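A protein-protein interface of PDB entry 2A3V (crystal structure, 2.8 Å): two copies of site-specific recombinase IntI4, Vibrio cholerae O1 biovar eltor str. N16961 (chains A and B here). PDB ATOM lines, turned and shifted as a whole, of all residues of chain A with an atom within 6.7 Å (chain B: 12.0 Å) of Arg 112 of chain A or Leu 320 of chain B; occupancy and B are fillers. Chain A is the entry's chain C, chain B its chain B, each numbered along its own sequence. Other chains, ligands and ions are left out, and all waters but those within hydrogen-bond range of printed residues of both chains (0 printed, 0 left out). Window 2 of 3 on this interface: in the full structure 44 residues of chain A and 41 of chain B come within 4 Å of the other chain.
The backbone carbonyl oxygen of Arg 112 of chain A lies close to the side-chain carboxylate of Glu 116 of chain A (2.7 Å). The backbone NH (N) of Leu 317 of chain B lies close to the side-chain hydroxyl (OG) of Ser 315 of chain B, at 3.1 Å. A ring nitrogen (ND1) of His 276 of chain A is in hydrogen-bond range of the side-chain hydroxyl of Tyr 130 of chain A (2.5 Å). The guanidinium group of Arg 112 of chain A lies within salt-bridge range of the side-chain carboxylate of Asp 109 of chain A, at 2.8 Å.
Among the printed residues, merely in contact across the chains: Arg 108 of chain A with Leu 320 of chain B, Arg 112 of chain A with Leu 320 of chain B, Leu 115 of chain A with Leu 317 of chain B, Tyr 130 of chain A with Pro 316 of chain B and Tyr 130 of chain A with Leu 317 of chain B.
Arg 108 of chain A touches just one residue of chain B: Leu 320. No residue of chain B comes within 4 Å of Asp 109 of chain A. No residue of chain B comes within 4 Å of Ile 111 of chain A. Of chain B, only Leu 320 comes within 4 Å of Arg 112 of chain A. No residue of chain B comes within 4 Å of Arg 113 of chain A. No residue of chain B comes within 4 Å of Leu 114 of chain A. Of chain B, only Leu 317 (3.6 Å) comes within 4 Å of Leu 115 of chain A. Of the printed residues of chain B, Tyr 130 of chain A touches Pro 316 (3.4 Å) and Leu 317 (3.8 Å). Of the printed residues of chain A, Pro 316 of chain B touches Tyr 130. Of the printed residues of chain A, Leu 317 of chain B touches Leu 115 (3.6 Å) and Tyr 130 (3.8 Å). The nearest residue of chain B that does not touch Arg 112 of chain A is Arg 319 of chain B (5.5 Å). The nearest residue of chain A that does not touch Leu 320 of chain B is Tyr 130 of chain A (4.2 Å).
Hydrophobic or aromatic side chains of chain A that line the printed part of chain B: Leu 115 and Tyr 130. Printed residues of chain B that touch a printed residue of chain A: Pro 316, Leu 317 and Leu 320. Hydrophobic or aromatic side chains of chain B within 4 Å of the printed part of chain A: Pro 316, Leu 317 and Leu 320. Among the printed residues, no Asp or Glu carboxylate lies within 4 Å of a Lys or Arg side-chain nitrogen of the other chain.
No position is printed for both chains. Of the 5 pairs that touch across the chains among the printed residues, none has its exchanged pair printed and touching as well.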
ATOM      1  N   THR A 107      15.975 -11.525  -9.962  1.00  0.00           N
ATOM      2  CA  THR A 107      15.177 -12.553 -10.612  1.00  0.00           C
ATOM      3  C   THR A 107      14.425 -11.939 -11.780  1.00  0.00           C
ATOM      4  O   THR A 107      14.225 -10.724 -11.842  1.00  0.00           O
ATOM      5  CB  THR A 107      14.133 -13.153  -9.656  1.00  0.00           C
ATOM      6  OG1 THR A 107      13.178 -12.143  -9.289  1.00  0.00           O
ATOM      7  CG2 THR A 107      14.807 -13.699  -8.406  1.00  0.00           C
ATOM      8  N   ARG A 108      14.005 -12.792 -12.702  1.00  0.00           N
ATOM      9  CA  ARG A 108      13.276 -12.345 -13.877  1.00  0.00           C
ATOM     10  C   ARG A 108      12.314 -11.223 -13.556  1.00  0.00           C
ATOM     11  O   ARG A 108      12.451 -10.112 -14.065  1.00  0.00           O
ATOM     12  CB  ARG A 108      12.477 -13.492 -14.469  1.00  0.00           C
ATOM     13  CG  ARG A 108      13.319 -14.619 -14.951  1.00  0.00           C
ATOM     14  CD  ARG A 108      14.105 -14.199 -16.152  1.00  0.00           C
ATOM     15  NE  ARG A 108      15.029 -15.255 -16.516  1.00  0.00           N
ATOM     16  CZ  ARG A 108      14.658 -16.455 -16.935  1.00  0.00           C
ATOM     17  NH1 ARG A 108      13.366 -16.747 -17.052  1.00  0.00           N
ATOM     18  NH2 ARG A 108      15.585 -17.367 -17.213  1.00  0.00           N
ATOM     19  N   ASP A 109      11.336 -11.522 -12.703  1.00  0.00           N
ATOM     20  CA  ASP A 109      10.322 -10.538 -12.351  1.00  0.00           C
ATOM     21  C   ASP A 109      10.907  -9.327 -11.647  1.00  0.00           C
ATOM     22  O   ASP A 109      10.447  -8.202 -11.847  1.00  0.00           O
ATOM     23  CB  ASP A 109       9.232 -11.172 -11.486  1.00  0.00           C
ATOM     24  CG  ASP A 109       7.953 -10.348 -11.476  1.00  0.00           C
ATOM     25  OD1 ASP A 109       7.867  -9.368 -10.692  1.00  0.00           O
ATOM     26  OD2 ASP A 109       7.040 -10.674 -12.274  1.00  0.00           O
ATOM     27  N   GLU A 110      11.919  -9.553 -10.821  1.00  0.00           N
ATOM     28  CA  GLU A 110      12.543  -8.449 -10.133  1.00  0.00           C
ATOM     29  C   GLU A 110      13.101  -7.498 -11.180  1.00  0.00           C
ATOM     30  O   GLU A 110      12.765  -6.313 -11.193  1.00  0.00           O
ATOM     31  CB  GLU A 110      13.649  -8.955  -9.207  1.00  0.00           C
ATOM     32  CG  GLU A 110      13.136  -9.550  -7.909  1.00  0.00           C
ATOM     33  CD  GLU A 110      14.255  -9.929  -6.955  1.00  0.00           C
ATOM     34  OE1 GLU A 110      13.967 -10.315  -5.795  1.00  0.00           O
ATOM     35  OE2 GLU A 110      15.433  -9.848  -7.367  1.00  0.00           O
ATOM     36  N   ILE A 111      13.937  -8.021 -12.074  1.00  0.00           N
ATOM     37  CA  ILE A 111      14.530  -7.191 -13.125  1.00  0.00           C
ATOM     38  C   ILE A 111      13.428  -6.599 -13.982  1.00  0.00           C
ATOM     39  O   ILE A 111      13.483  -5.433 -14.369  1.00  0.00           O
ATOM     40  CB  ILE A 111      15.488  -8.008 -14.020  1.00  0.00           C
ATOM     41  CG1 ILE A 111      16.690  -8.437 -13.193  1.00  0.00           C
ATOM     42  CG2 ILE A 111      15.961  -7.177 -15.211  1.00  0.00           C
ATOM     43  CD1 ILE A 111      17.594  -9.362 -13.901  1.00  0.00           C
ATOM     44  N   ARG A 112      12.427  -7.418 -14.268  1.00  0.00           N
ATOM     45  CA  ARG A 112      11.294  -6.985 -15.062  1.00  0.00           C
ATOM     46  C   ARG A 112      10.674  -5.736 -14.433  1.00  0.00           C
ATOM     47  O   ARG A 112      10.356  -4.774 -15.130  1.00  0.00           O
ATOM     48  CB  ARG A 112      10.263  -8.115 -15.145  1.00  0.00           C
ATOM     49  CG  ARG A 112       8.951  -7.759 -15.851  1.00  0.00           C
ATOM     50  CD  ARG A 112       8.686  -8.653 -17.062  1.00  0.00           C
ATOM     51  NE  ARG A 112       9.029 -10.059 -16.826  1.00  0.00           N
ATOM     52  CZ  ARG A 112       8.550 -10.802 -15.829  1.00  0.00           C
ATOM     53  NH1 ARG A 112       7.692 -10.275 -14.956  1.00  0.00           N
ATOM     54  NH2 ARG A 112       8.933 -12.072 -15.700  1.00  0.00           N
ATOM     55  N   ARG A 113      10.519  -5.747 -13.113  1.00  0.00           N
ATOM     56  CA  ARG A 113       9.926  -4.609 -12.422  1.00  0.00           C
ATOM     57  C   ARG A 113      10.915  -3.473 -12.266  1.00  0.00           C
ATOM     58  O   ARG A 113      10.532  -2.308 -12.194  1.00  0.00           O
ATOM     59  CB  ARG A 113       9.393  -5.037 -11.054  1.00  0.00           C
ATOM     60  CG  ARG A 113       8.343  -6.124 -11.163  1.00  0.00           C
ATOM     61  CD  ARG A 113       7.651  -6.418  -9.846  1.00  0.00           C
ATOM     62  NE  ARG A 113       8.525  -7.012  -8.835  1.00  0.00           N
ATOM     63  CZ  ARG A 113       9.037  -6.346  -7.801  1.00  0.00           C
ATOM     64  NH1 ARG A 113       8.769  -5.052  -7.640  1.00  0.00           N
ATOM     65  NH2 ARG A 113       9.794  -6.979  -6.912  1.00  0.00           N
ATOM     66  N   LEU A 114      12.193  -3.817 -12.229  1.00  0.00           N
ATOM     67  CA  LEU A 114      13.228  -2.813 -12.083  1.00  0.00           C
ATOM     68  C   LEU A 114      13.297  -1.921 -13.320  1.00  0.00           C
ATOM     69  O   LEU A 114      13.415  -0.702 -13.205  1.00  0.00           O
ATOM     70  CB  LEU A 114      14.578  -3.498 -11.832  1.00  0.00           C
ATOM     71  CG  LEU A 114      15.828  -2.660 -11.522  1.00  0.00           C
ATOM     72  CD1 LEU A 114      16.432  -2.131 -12.797  1.00  0.00           C
ATOM     73  CD2 LEU A 114      15.474  -1.519 -10.592  1.00  0.00           C
ATOM     74  N   LEU A 115      13.199  -2.525 -14.500  1.00  0.00           N
ATOM     75  CA  LEU A 115      13.274  -1.774 -15.754  1.00  0.00           C
ATOM     76  C   LEU A 115      12.048  -0.907 -16.000  1.00  0.00           C
ATOM     77  O   LEU A 115      11.970  -0.175 -16.991  1.00  0.00           O
ATOM     78  CB  LEU A 115      13.456  -2.741 -16.922  1.00  0.00           C
ATOM     79  CG  LEU A 115      14.727  -3.591 -16.841  1.00  0.00           C
ATOM     80  CD1 LEU A 115      14.662  -4.724 -17.847  1.00  0.00           C
ATOM     81  CD2 LEU A 115      15.943  -2.710 -17.082  1.00  0.00           C
ATOM     82  N   GLU A 116      11.097  -0.983 -15.082  1.00  0.00           N
ATOM     83  CA  GLU A 116       9.870  -0.226 -15.214  1.00  0.00           C
ATOM     84  C   GLU A 116       9.985   1.194 -14.714  1.00  0.00           C
ATOM     85  O   GLU A 116      10.021   2.135 -15.504  1.00  0.00           O
ATOM     86  CB  GLU A 116       8.744  -0.942 -14.477  1.00  0.00           C
ATOM     87  CG  GLU A 116       8.534  -2.349 -14.986  1.00  0.00           C
ATOM     88  CD  GLU A 116       8.576  -2.407 -16.502  1.00  0.00           C
ATOM     89  OE1 GLU A 116       7.789  -1.670 -17.149  1.00  0.00           O
ATOM     90  OE2 GLU A 116       9.401  -3.180 -17.047  1.00  0.00           O
ATOM     91  N   ILE A 117      10.038   1.344 -13.396  1.00  0.00           N
ATOM     92  CA  ILE A 117      10.123   2.664 -12.785  1.00  0.00           C
ATOM     93  C   ILE A 117      11.412   3.421 -13.070  1.00  0.00           C
ATOM     94  O   ILE A 117      11.890   4.186 -12.235  1.00  0.00           O
ATOM     95  CB  ILE A 117       9.907   2.589 -11.253  1.00  0.00           C
ATOM     96  CG1 ILE A 117      10.446   1.266 -10.706  1.00  0.00           C
ATOM     97  CG2 ILE A 117       8.427   2.748 -10.934  1.00  0.00           C
ATOM     98  CD1 ILE A 117      11.919   1.059 -10.956  1.00  0.00           C
ATOM     99  N   TYR A 130      22.028  -5.430 -18.491  1.00  0.00           N
ATOM    100  CA  TYR A 130      21.435  -6.726 -18.230  1.00  0.00           C
ATOM    101  C   TYR A 130      21.291  -7.530 -19.513  1.00  0.00           C
ATOM    102  O   TYR A 130      21.516  -8.738 -19.528  1.00  0.00           O
ATOM    103  CB  TYR A 130      20.064  -6.551 -17.570  1.00  0.00           C
ATOM    104  CG  TYR A 130      19.278  -7.835 -17.475  1.00  0.00           C
ATOM    105  CD1 TYR A 130      19.754  -8.905 -16.725  1.00  0.00           C
ATOM    106  CD2 TYR A 130      18.080  -8.001 -18.175  1.00  0.00           C
ATOM    107  CE1 TYR A 130      19.062 -10.108 -16.681  1.00  0.00           C
ATOM    108  CE2 TYR A 130      17.380  -9.202 -18.131  1.00  0.00           C
ATOM    109  CZ  TYR A 130      17.878 -10.248 -17.384  1.00  0.00           C
ATOM    110  OH  TYR A 130      17.219 -11.456 -17.326  1.00  0.00           O
ATOM    111  N   HIS A 276      20.993 -15.704 -15.451  1.00  0.00           N
ATOM    112  CA  HIS A 276      19.846 -16.045 -16.261  1.00  0.00           C
ATOM    113  C   HIS A 276      20.156 -16.885 -17.491  1.00  0.00           C
ATOM    114  O   HIS A 276      19.408 -17.805 -17.793  1.00  0.00           O
ATOM    115  CB  HIS A 276      19.088 -14.777 -16.605  1.00  0.00           C
ATOM    116  CG  HIS A 276      18.420 -14.168 -15.413  1.00  0.00           C
ATOM    117  ND1 HIS A 276      17.748 -12.964 -15.461  1.00  0.00           N
ATOM    118  CD2 HIS A 276      18.331 -14.599 -14.131  1.00  0.00           C
ATOM    119  CE1 HIS A 276      17.276 -12.680 -14.257  1.00  0.00           C
ATOM    120  NE2 HIS A 276      17.618 -13.657 -13.433  1.00  0.00           N
ATOM    121  N   LEU B 314      20.788 -15.867 -27.144  1.00  0.00           N
ATOM    122  CA  LEU B 314      19.653 -15.013 -26.941  1.00  0.00           C
ATOM    123  C   LEU B 314      19.759 -14.167 -25.675  1.00  0.00           C
ATOM    124  O   LEU B 314      19.839 -14.698 -24.562  1.00  0.00           O
ATOM    125  CB  LEU B 314      18.401 -15.864 -26.901  1.00  0.00           C
ATOM    126  CG  LEU B 314      17.133 -15.032 -26.805  1.00  0.00           C
ATOM    127  CD1 LEU B 314      16.962 -14.190 -28.061  1.00  0.00           C
ATOM    128  CD2 LEU B 314      15.964 -15.968 -26.602  1.00  0.00           C
ATOM    129  N   SER B 315      19.746 -12.849 -25.847  1.00  0.00           N
ATOM    130  CA  SER B 315      19.842 -11.944 -24.711  1.00  0.00           C
ATOM    131  C   SER B 315      18.791 -12.242 -23.648  1.00  0.00           C
ATOM    132  O   SER B 315      17.635 -12.469 -23.974  1.00  0.00           O
ATOM    133  CB  SER B 315      19.667 -10.507 -25.167  1.00  0.00           C
ATOM    134  OG  SER B 315      19.401  -9.696 -24.035  1.00  0.00           O
ATOM    135  N   PRO B 316      19.176 -12.251 -22.364  1.00  0.00           N
ATOM    136  CA  PRO B 316      18.199 -12.528 -21.307  1.00  0.00           C
ATOM    137  C   PRO B 316      17.094 -11.469 -21.293  1.00  0.00           C
ATOM    138  O   PRO B 316      15.984 -11.725 -20.834  1.00  0.00           O
ATOM    139  CB  PRO B 316      19.041 -12.491 -20.037  1.00  0.00           C
ATOM    140  CG  PRO B 316      20.373 -12.958 -20.506  1.00  0.00           C
ATOM    141  CD  PRO B 316      20.542 -12.211 -21.819  1.00  0.00           C
ATOM    142  N   LEU B 317      17.408 -10.278 -21.790  1.00  0.00           N
ATOM    143  CA  LEU B 317      16.432  -9.200 -21.838  1.00  0.00           C
ATOM    144  C   LEU B 317      15.366  -9.529 -22.869  1.00  0.00           C
ATOM    145  O   LEU B 317      14.262  -9.006 -22.816  1.00  0.00           O
ATOM    146  CB  LEU B 317      17.099  -7.885 -22.225  1.00  0.00           C
ATOM    147  CG  LEU B 317      16.156  -6.689 -22.349  1.00  0.00           C
ATOM    148  CD1 LEU B 317      15.656  -6.282 -20.970  1.00  0.00           C
ATOM    149  CD2 LEU B 317      16.887  -5.539 -22.992  1.00  0.00           C
ATOM    150  N   SER B 318      15.707 -10.386 -23.819  1.00  0.00           N
ATOM    151  CA  SER B 318      14.758 -10.764 -24.847  1.00  0.00           C
ATOM    152  C   SER B 318      13.735 -11.733 -24.315  1.00  0.00           C
ATOM    153  O   SER B 318      12.869 -12.184 -25.057  1.00  0.00           O
ATOM    154  CB  SER B 318      15.457 -11.407 -26.034  1.00  0.00           C
ATOM    155  OG  SER B 318      16.116 -10.440 -26.818  1.00  0.00           O
ATOM    156  N   ARG B 319      13.832 -12.081 -23.040  1.00  0.00           N
ATOM    157  CA  ARG B 319      12.845 -12.990 -22.479  1.00  0.00           C
ATOM    158  C   ARG B 319      12.030 -12.241 -21.428  1.00  0.00           C
ATOM    159  O   ARG B 319      10.864 -11.910 -21.649  1.00  0.00           O
ATOM    160  CB  ARG B 319      13.528 -14.200 -21.862  1.00  0.00           C
ATOM    161  CG  ARG B 319      14.575 -14.811 -22.759  1.00  0.00           C
ATOM    162  CD  ARG B 319      15.365 -15.850 -21.996  1.00  0.00           C
ATOM    163  NE  ARG B 319      14.803 -17.192 -22.118  1.00  0.00           N
ATOM    164  CZ  ARG B 319      15.177 -18.081 -23.036  1.00  0.00           C
ATOM    165  NH1 ARG B 319      16.120 -17.774 -23.921  1.00  0.00           N
ATOM    166  NH2 ARG B 319      14.621 -19.288 -23.060  1.00  0.00           N
ATOM    167  N   LEU B 320      12.647 -11.946 -20.293  1.00  0.00           N
ATOM    168  CA  LEU B 320      11.941 -11.234 -19.235  1.00  0.00           C
ATOM    169  C   LEU B 320      12.822 -10.075 -18.729  1.00  0.00           C
ATOM    170  O   LEU B 320      13.237 -10.079 -17.547  1.00  0.00           O
ATOM    171  CB  LEU B 320      11.570 -12.223 -18.089  1.00  0.00           C
ATOM    172  CG  LEU B 320      10.893 -13.594 -18.395  1.00  0.00           C
ATOM    173  CD1 LEU B 320      11.941 -14.585 -18.940  1.00  0.00           C
ATOM    174  CD2 LEU B 320      10.250 -14.190 -17.126  1.00  0.00           C
ATOM    175  OXT LEU B 320      13.096  -9.171 -19.541  1.00  0.00           O
